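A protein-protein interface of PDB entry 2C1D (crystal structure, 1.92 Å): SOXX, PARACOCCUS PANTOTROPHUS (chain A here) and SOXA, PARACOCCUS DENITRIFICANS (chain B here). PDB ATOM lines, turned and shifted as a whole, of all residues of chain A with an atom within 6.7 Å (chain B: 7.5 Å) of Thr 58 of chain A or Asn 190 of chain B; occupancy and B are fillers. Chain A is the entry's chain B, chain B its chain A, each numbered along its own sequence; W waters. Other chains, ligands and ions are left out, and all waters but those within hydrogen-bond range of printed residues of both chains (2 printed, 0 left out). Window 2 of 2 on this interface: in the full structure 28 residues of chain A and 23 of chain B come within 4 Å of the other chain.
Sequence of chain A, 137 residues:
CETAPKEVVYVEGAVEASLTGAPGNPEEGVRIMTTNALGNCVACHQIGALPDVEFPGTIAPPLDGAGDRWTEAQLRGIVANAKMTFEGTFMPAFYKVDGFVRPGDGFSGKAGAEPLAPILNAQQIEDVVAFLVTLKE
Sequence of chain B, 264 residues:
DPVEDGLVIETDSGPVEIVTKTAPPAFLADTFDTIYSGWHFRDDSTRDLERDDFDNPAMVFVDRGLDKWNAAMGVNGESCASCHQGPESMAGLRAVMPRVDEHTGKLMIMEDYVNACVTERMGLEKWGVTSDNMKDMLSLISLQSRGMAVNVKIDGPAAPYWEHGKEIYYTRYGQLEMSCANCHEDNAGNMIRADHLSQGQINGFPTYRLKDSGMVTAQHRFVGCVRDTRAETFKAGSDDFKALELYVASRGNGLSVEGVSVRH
Of the printed residues of chain B, Gly 57 of chain A touches Met 191. Thr 58 of chain A touches two residues of chain B. Of the printed residues of chain A, Asn 187 of chain B touches Ile 59 (3.6 Å). Asn 190 of chain B touches two residues of chain A. The nearest residue of chain B that does not touch Thr 58 of chain A is Ile 192 of chain B (5.2 Å). The nearest residue of chain A that does not touch Asn 190 of chain B is Ala 60 of chain A (6.2 Å). The nearest printed residue of chain B that does not touch Val 42 of chain A is Ile 192 of chain B (6.1 Å).
Water W1 bridges the backbone carbonyl oxygen of Arg 193 of chain B (2.7 Å) and the backbone carbonyl oxygen of Pro 56 of chain A (2.8 Å). Water W2 lies within hydrogen-bond range of the backbone carbonyl oxygen (O) of Thr 58 of chain A (2.9 Å) and the side-chain amide oxygen (OD1) of Asn 190 of chain B (3.5 Å).
Arg 193 of chain B touches Val 42 of chain A (CD to O, 3.7 Å). O of Met 191 of chain B touches O of Ala 43 of chain A, at 3.8 Å. Ile 192 of chain B touches Ala 43 of chain A (CA to O, 3.5 Å). Gly 57 of chain A touches Met 191 of chain B. Thr 58 of chain A touches Asn 190 of chain B. Asn 187 of chain B touches Ile 59 of chain A. CB of Asn 190 of chain B touches CD1 of Ile 59 of chain A, at 3.8 Å. Ile 59 of chain A touches Met 191 of chain B.
Hydrophobic or aromatic side chains of chain A that line the printed part of chain B: Val 42 and Ile 59. Of the 17 printed residues of chain B, 5 touch a printed residue of chain A.
The backbone NH of Leu 197 of chain B is in hydrogen-bond range of the backbone carbonyl oxygen of Asn 190 of chain B (2.9 Å). O of Val 42 of chain A is in hydrogen-bond range of N of Gly 57 of chain A (2.9 Å). The backbone carbonyl oxygen (O) of Cys 44 of chain A is in hydrogen-bond range of the backbone NH (N) of Ile 59 of chain A (3.1 Å). The side-chain amide oxygen (OD1) of Asn 187 of chain B sits at hydrogen-bond distance from the side-chain amide nitrogen (ND2) of Asn 190 of chain B, at 3.1 Å.
N of Met 191 of chain B lies within hydrogen-bond range of OG1 of Thr 58 of chain A. O of Ala 43 of chain A is in hydrogen-bond range of N of Arg 193 of chain B.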
ATOM      1  N   VAL A  42      23.933 -11.244  23.645  1.00  0.00           N
ATOM      2  CA  VAL A  42      22.853 -11.635  22.762  1.00  0.00           C
ATOM      3  C   VAL A  42      22.305 -13.033  23.022  1.00  0.00           C
ATOM      4  O   VAL A  42      21.270 -13.380  22.448  1.00  0.00           O
ATOM      5  CB  VAL A  42      23.227 -11.487  21.257  1.00  0.00           C
ATOM      6  CG1 VAL A  42      23.452 -10.015  20.888  1.00  0.00           C
ATOM      7  CG2 VAL A  42      24.436 -12.306  20.895  1.00  0.00           C
ATOM      8  N   ALA A  43      22.933 -13.824  23.901  1.00  0.00           N
ATOM      9  CA  ALA A  43      22.341 -15.099  24.306  1.00  0.00           C
ATOM     10  C   ALA A  43      21.066 -14.841  25.080  1.00  0.00           C
ATOM     11  O   ALA A  43      20.133 -15.622  24.992  1.00  0.00           O
ATOM     12  CB  ALA A  43      23.292 -15.961  25.150  1.00  0.00           C
ATOM     13  N   CYS A  44      21.028 -13.735  25.830  1.00  0.00           N
ATOM     14  CA  CYS A  44      19.870 -13.385  26.652  1.00  0.00           C
ATOM     15  C   CYS A  44      19.064 -12.172  26.175  1.00  0.00           C
ATOM     16  O   CYS A  44      17.849 -12.141  26.402  1.00  0.00           O
ATOM     17  CB  CYS A  44      20.324 -13.153  28.086  1.00  0.00           C
ATOM     18  SG  CYS A  44      21.000 -14.647  28.825  1.00  0.00           S
ATOM     19  N   HIS A  45      19.726 -11.200  25.528  1.00  0.00           N
ATOM     20  CA  HIS A  45      19.124  -9.932  25.072  1.00  0.00           C
ATOM     21  C   HIS A  45      19.104  -9.769  23.565  1.00  0.00           C
ATOM     22  O   HIS A  45      20.101 -10.007  22.886  1.00  0.00           O
ATOM     23  CB  HIS A  45      19.921  -8.702  25.558  1.00  0.00           C
ATOM     24  CG  HIS A  45      20.023  -8.552  27.044  1.00  0.00           C
ATOM     25  ND1 HIS A  45      19.272  -9.280  27.928  1.00  0.00           N
ATOM     26  CD2 HIS A  45      20.806  -7.754  27.801  1.00  0.00           C
ATOM     27  CE1 HIS A  45      19.593  -8.936  29.162  1.00  0.00           C
ATOM     28  NE2 HIS A  45      20.535  -8.030  29.114  1.00  0.00           N
ATOM     29  N   GLN A  46      17.990  -9.271  23.047  1.00  0.00           N
ATOM     30  CA  GLN A  46      17.939  -8.790  21.676  1.00  0.00           C
ATOM     31  C   GLN A  46      18.606  -7.416  21.624  1.00  0.00           C
ATOM     32  O   GLN A  46      18.602  -6.691  22.601  1.00  0.00           O
ATOM     33  CB  GLN A  46      16.488  -8.635  21.205  1.00  0.00           C
ATOM     34  CG  GLN A  46      15.807  -9.921  20.764  1.00  0.00           C
ATOM     35  CD  GLN A  46      14.270  -9.785  20.682  1.00  0.00           C
ATOM     36  OE1 GLN A  46      13.727  -8.684  20.866  1.00  0.00           O
ATOM     37  NE2 GLN A  46      13.575 -10.904  20.413  1.00  0.00           N
ATOM     38  N   PRO A  56      19.063 -14.054  18.621  1.00  0.00           N
ATOM     39  CA  PRO A  56      19.080 -13.315  19.899  1.00  0.00           C
ATOM     40  C   PRO A  56      18.115 -13.949  20.881  1.00  0.00           C
ATOM     41  O   PRO A  56      17.063 -14.429  20.470  1.00  0.00           O
ATOM     42  CB  PRO A  56      18.602 -11.925  19.512  1.00  0.00           C
ATOM     43  CG  PRO A  56      17.780 -12.161  18.268  1.00  0.00           C
ATOM     44  CD  PRO A  56      18.473 -13.254  17.527  1.00  0.00           C
ATOM     45  N   GLY A  57      18.462 -13.953  22.162  1.00  0.00           N
ATOM     46  CA  GLY A  57      17.646 -14.602  23.163  1.00  0.00           C
ATOM     47  C   GLY A  57      16.457 -13.756  23.573  1.00  0.00           C
ATOM     48  O   GLY A  57      16.348 -12.597  23.162  1.00  0.00           O
ATOM     49  N   THR A  58      15.592 -14.339  24.392  1.00  0.00           N
ATOM     50  CA  THR A  58      14.403 -13.672  24.919  1.00  0.00           C
ATOM     51  C   THR A  58      14.338 -13.822  26.417  1.00  0.00           C
ATOM     52  O   THR A  58      13.255 -13.748  27.005  1.00  0.00           O
ATOM     53  CB  THR A  58      13.106 -14.248  24.299  1.00  0.00           C
ATOM     54  OG1 THR A  58      13.086 -15.682  24.423  1.00  0.00           O
ATOM     55  CG2 THR A  58      13.057 -13.988  22.805  1.00  0.00           C
ATOM     56  N   ILE A  59      15.495 -14.024  27.042  1.00  0.00           N
ATOM     57  CA  ILE A  59      15.583 -14.145  28.494  1.00  0.00           C
ATOM     58  C   ILE A  59      15.253 -12.795  29.164  1.00  0.00           C
ATOM     59  O   ILE A  59      14.576 -12.735  30.198  1.00  0.00           O
ATOM     60  CB  ILE A  59      17.005 -14.584  28.882  1.00  0.00           C
ATOM     61  CG1 ILE A  59      17.333 -15.991  28.334  1.00  0.00           C
ATOM     62  CG2 ILE A  59      17.257 -14.488  30.406  1.00  0.00           C
ATOM     63  CD1 ILE A  59      16.473 -17.125  28.853  1.00  0.00           C
ATOM     64  N   ALA A  60      15.768 -11.723  28.582  1.00  0.00           N
ATOM     65  CA  ALA A  60      15.559 -10.402  29.145  1.00  0.00           C
ATOM     66  C   ALA A  60      15.206  -9.427  28.052  1.00  0.00           C
ATOM     67  O   ALA A  60      15.467  -9.688  26.886  1.00  0.00           O
ATOM     68  CB  ALA A  60      16.803  -9.970  29.863  1.00  0.00           C
ATOM     69  N   PRO A  61      14.606  -8.293  28.416  1.00  0.00           N
ATOM     70  CA  PRO A  61      14.227  -7.276  27.426  1.00  0.00           C
ATOM     71  C   PRO A  61      15.394  -6.786  26.542  1.00  0.00           C
ATOM     72  O   PRO A  61      16.575  -6.861  26.945  1.00  0.00           O
ATOM     73  CB  PRO A  61      13.678  -6.129  28.299  1.00  0.00           C
ATOM     74  CG  PRO A  61      13.171  -6.808  29.534  1.00  0.00           C
ATOM     75  CD  PRO A  61      14.225  -7.896  29.785  1.00  0.00           C
ATOM     76  N   ASP B   1       8.150 -20.862  23.861  1.00  0.00           N
ATOM     77  CA  ASP B   1       6.993 -21.478  24.626  1.00  0.00           C
ATOM     78  C   ASP B   1       6.586 -22.858  24.089  1.00  0.00           C
ATOM     79  O   ASP B   1       6.743 -23.108  22.897  1.00  0.00           O
ATOM     80  CB  ASP B   1       5.746 -20.584  24.551  1.00  0.00           C
ATOM     81  CG  ASP B   1       5.671 -19.576  25.674  1.00  0.00           C
ATOM     82  OD1 ASP B   1       6.740 -19.179  26.206  1.00  0.00           O
ATOM     83  OD2 ASP B   1       4.581 -19.114  26.083  1.00  0.00           O
ATOM     84  N   PRO B   2       6.012 -23.731  24.927  1.00  0.00           N
ATOM     85  CA  PRO B   2       5.700 -25.110  24.499  1.00  0.00           C
ATOM     86  C   PRO B   2       4.566 -25.213  23.459  1.00  0.00           C
ATOM     87  O   PRO B   2       3.515 -24.594  23.605  1.00  0.00           O
ATOM     88  CB  PRO B   2       5.312 -25.820  25.807  1.00  0.00           C
ATOM     89  CG  PRO B   2       4.867 -24.722  26.724  1.00  0.00           C
ATOM     90  CD  PRO B   2       5.627 -23.490  26.334  1.00  0.00           C
ATOM     91  N   PHE B  41       9.181 -28.613  23.146  1.00  0.00           N
ATOM     92  CA  PHE B  41       9.990 -27.427  22.856  1.00  0.00           C
ATOM     93  C   PHE B  41      10.855 -27.595  21.611  1.00  0.00           C
ATOM     94  O   PHE B  41      11.666 -26.729  21.284  1.00  0.00           O
ATOM     95  CB  PHE B  41      10.872 -27.133  24.069  1.00  0.00           C
ATOM     96  CG  PHE B  41      10.093 -26.898  25.324  1.00  0.00           C
ATOM     97  CD1 PHE B  41       9.694 -27.953  26.109  1.00  0.00           C
ATOM     98  CD2 PHE B  41       9.763 -25.611  25.725  1.00  0.00           C
ATOM     99  CE1 PHE B  41       8.964 -27.742  27.252  1.00  0.00           C
ATOM    100  CE2 PHE B  41       9.045 -25.395  26.887  1.00  0.00           C
ATOM    101  CZ  PHE B  41       8.634 -26.448  27.636  1.00  0.00           C
ATOM    102  N   CYS B 183      17.659 -21.803  34.532  1.00  0.00           N
ATOM    103  CA  CYS B 183      17.350 -22.024  33.131  1.00  0.00           C
ATOM    104  C   CYS B 183      16.049 -22.792  32.885  1.00  0.00           C
ATOM    105  O   CYS B 183      15.182 -22.315  32.140  1.00  0.00           O
ATOM    106  CB  CYS B 183      18.514 -22.729  32.463  1.00  0.00           C
ATOM    107  SG  CYS B 183      19.948 -21.645  32.395  1.00  0.00           S
ATOM    108  N   ASP B 186      12.955 -21.064  35.799  1.00  0.00           N
ATOM    109  CA  ASP B 186      12.643 -19.640  35.623  1.00  0.00           C
ATOM    110  C   ASP B 186      12.461 -19.260  34.181  1.00  0.00           C
ATOM    111  O   ASP B 186      11.781 -18.283  33.893  1.00  0.00           O
ATOM    112  CB  ASP B 186      13.752 -18.747  36.199  1.00  0.00           C
ATOM    113  CG  ASP B 186      13.875 -18.856  37.696  1.00  0.00           C
ATOM    114  OD1 ASP B 186      12.961 -19.422  38.359  1.00  0.00           O
ATOM    115  OD2 ASP B 186      14.877 -18.417  38.295  1.00  0.00           O
ATOM    116  N   ASN B 187      13.087 -19.997  33.264  1.00  0.00           N
ATOM    117  CA  ASN B 187      13.137 -19.566  31.876  1.00  0.00           C
ATOM    118  C   ASN B 187      12.658 -20.578  30.825  1.00  0.00           C
ATOM    119  O   ASN B 187      12.923 -20.395  29.643  1.00  0.00           O
ATOM    120  CB  ASN B 187      14.541 -19.063  31.529  1.00  0.00           C
ATOM    121  CG  ASN B 187      14.819 -17.697  32.095  1.00  0.00           C
ATOM    122  OD1 ASN B 187      14.269 -16.700  31.620  1.00  0.00           O
ATOM    123  ND2 ASN B 187      15.639 -17.641  33.137  1.00  0.00           N
ATOM    124  N   ALA B 188      11.932 -21.600  31.255  1.00  0.00           N
ATOM    125  CA  ALA B 188      11.312 -22.558  30.341  1.00  0.00           C
ATOM    126  C   ALA B 188      10.400 -21.797  29.412  1.00  0.00           C
ATOM    127  O   ALA B 188       9.637 -20.946  29.865  1.00  0.00           O
ATOM    128  CB  ALA B 188      10.518 -23.597  31.113  1.00  0.00           C
ATOM    129  N   GLY B 189      10.533 -22.057  28.119  1.00  0.00           N
ATOM    130  CA  GLY B 189       9.747 -21.399  27.097  1.00  0.00           C
ATOM    131  C   GLY B 189      10.490 -20.272  26.399  1.00  0.00           C
ATOM    132  O   GLY B 189      10.103 -19.849  25.292  1.00  0.00           O
ATOM    133  N   ASN B 190      11.553 -19.779  27.032  1.00  0.00           N
ATOM    134  CA  ASN B 190      12.362 -18.715  26.449  1.00  0.00           C
ATOM    135  C   ASN B 190      13.467 -19.255  25.564  1.00  0.00           C
ATOM    136  O   ASN B 190      13.749 -20.459  25.572  1.00  0.00           O
ATOM    137  CB  ASN B 190      12.922 -17.817  27.559  1.00  0.00           C
ATOM    138  CG  ASN B 190      11.803 -17.005  28.277  1.00  0.00           C
ATOM    139  OD1 ASN B 190      10.743 -16.735  27.692  1.00  0.00           O
ATOM    140  ND2 ASN B 190      12.054 -16.601  29.506  1.00  0.00           N
ATOM    141  N   MET B 191      14.068 -18.349  24.787  1.00  0.00           N
ATOM    142  CA  MET B 191      15.190 -18.664  23.932  1.00  0.00           C
ATOM    143  C   MET B 191      16.464 -18.214  24.623  1.00  0.00           C
ATOM    144  O   MET B 191      16.589 -17.052  25.024  1.00  0.00           O
ATOM    145  CB  MET B 191      15.058 -17.953  22.588  1.00  0.00           C
ATOM    146  CG  MET B 191      13.851 -18.357  21.764  1.00  0.00           C
ATOM    147  SD  MET B 191      13.728 -20.112  21.370  1.00  0.00           S
ATOM    148  CE  MET B 191      15.160 -20.349  20.357  1.00  0.00           C
ATOM    149  N   ILE B 192      17.390 -19.149  24.808  1.00  0.00           N
ATOM    150  CA  ILE B 192      18.748 -18.807  25.156  1.00  0.00           C
ATOM    151  C   ILE B 192      19.585 -19.062  23.916  1.00  0.00           C
ATOM    152  O   ILE B 192      19.805 -20.207  23.507  1.00  0.00           O
ATOM    153  CB  ILE B 192      19.210 -19.555  26.469  1.00  0.00           C
ATOM    154  CG1 ILE B 192      20.477 -18.929  27.047  1.00  0.00           C
ATOM    155  CG2 ILE B 192      19.399 -21.055  26.267  1.00  0.00           C
ATOM    156  CD1 ILE B 192      20.497 -19.010  28.566  1.00  0.00           C
ATOM    157  N   ARG B 193      20.030 -17.958  23.319  1.00  0.00           N
ATOM    158  CA  ARG B 193      20.481 -17.907  21.950  1.00  0.00           C
ATOM    159  C   ARG B 193      19.546 -18.784  21.063  1.00  0.00           C
ATOM    160  O   ARG B 193      18.332 -18.567  21.076  1.00  0.00           O
ATOM    161  CB  ARG B 193      21.993 -18.231  21.846  1.00  0.00           C
ATOM    162  CG  ARG B 193      22.658 -17.661  20.580  1.00  0.00           C
ATOM    163  CD  ARG B 193      22.786 -16.141  20.601  1.00  0.00           C
ATOM    164  NE  ARG B 193      23.159 -15.559  19.307  1.00  0.00           N
ATOM    165  CZ  ARG B 193      24.420 -15.416  18.882  1.00  0.00           C
ATOM    166  NH1 ARG B 193      25.422 -15.801  19.631  1.00  0.00           N
ATOM    167  NH2 ARG B 193      24.676 -14.863  17.698  1.00  0.00           N
ATOM    168  N   ALA B 194      20.094 -19.762  20.340  1.00  0.00           N
ATOM    169  CA  ALA B 194      19.307 -20.567  19.414  1.00  0.00           C
ATOM    170  C   ALA B 194      18.556 -21.719  20.061  1.00  0.00           C
ATOM    171  O   ALA B 194      17.795 -22.404  19.380  1.00  0.00           O
ATOM    172  CB  ALA B 194      20.195 -21.095  18.276  1.00  0.00           C
ATOM    173  N   ASP B 195      18.745 -21.942  21.361  1.00  0.00           N
ATOM    174  CA  ASP B 195      18.040 -23.029  22.064  1.00  0.00           C
ATOM    175  C   ASP B 195      16.759 -22.594  22.781  1.00  0.00           C
ATOM    176  O   ASP B 195      16.775 -21.641  23.545  1.00  0.00           O
ATOM    177  CB  ASP B 195      18.954 -23.676  23.105  1.00  0.00           C
ATOM    178  CG  ASP B 195      20.160 -24.341  22.491  1.00  0.00           C
ATOM    179  OD1 ASP B 195      19.980 -25.169  21.561  1.00  0.00           O
ATOM    180  OD2 ASP B 195      21.326 -24.078  22.891  1.00  0.00           O
ATOM    181  N   HIS B 196      15.680 -23.333  22.548  1.00  0.00           N
ATOM    182  CA  HIS B 196      14.375 -23.147  23.198  1.00  0.00           C
ATOM    183  C   HIS B 196      14.429 -23.958  24.479  1.00  0.00           C
ATOM    184  O   HIS B 196      14.520 -25.194  24.422  1.00  0.00           O
ATOM    185  CB  HIS B 196      13.280 -23.731  22.287  1.00  0.00           C
ATOM    186  CG  HIS B 196      11.878 -23.361  22.664  1.00  0.00           C
ATOM    187  ND1 HIS B 196      10.789 -23.898  22.013  1.00  0.00           N
ATOM    188  CD2 HIS B 196      11.381 -22.480  23.573  1.00  0.00           C
ATOM    189  CE1 HIS B 196       9.682 -23.359  22.497  1.00  0.00           C
ATOM    190  NE2 HIS B 196      10.012 -22.508  23.454  1.00  0.00           N
ATOM    191  N   LEU B 197      14.396 -23.263  25.624  1.00  0.00           N
ATOM    192  CA  LEU B 197      14.555 -23.897  26.900  1.00  0.00           C
ATOM    193  C   LEU B 197      13.338 -24.737  27.272  1.00  0.00           C
ATOM    194  O   LEU B 197      12.198 -24.253  27.258  1.00  0.00           O
ATOM    195  CB  LEU B 197      14.812 -22.869  28.005  1.00  0.00           C
ATOM    196  CG  LEU B 197      16.273 -22.480  28.188  1.00  0.00           C
ATOM    197  CD1 LEU B 197      16.389 -21.185  29.000  1.00  0.00           C
ATOM    198  CD2 LEU B 197      17.104 -23.610  28.813  1.00  0.00           C
ATOM    199  N   SER B 198      13.606 -25.981  27.650  1.00  0.00           N
ATOM    200  CA  SER B 198      12.574 -26.891  28.184  1.00  0.00           C
ATOM    201  C   SER B 198      12.591 -26.870  29.707  1.00  0.00           C
ATOM    202  O   SER B 198      13.279 -26.041  30.319  1.00  0.00           O
ATOM    203  CB  SER B 198      12.814 -28.302  27.642  1.00  0.00           C
ATOM    204  OG  SER B 198      13.899 -28.911  28.270  1.00  0.00           O
HETATM  205  O   HOH W   1      16.886 -17.025  19.387  1.00  0.00           O
HETATM  206  O   HOH W   2      10.401 -13.309  27.349  1.00  0.00           O
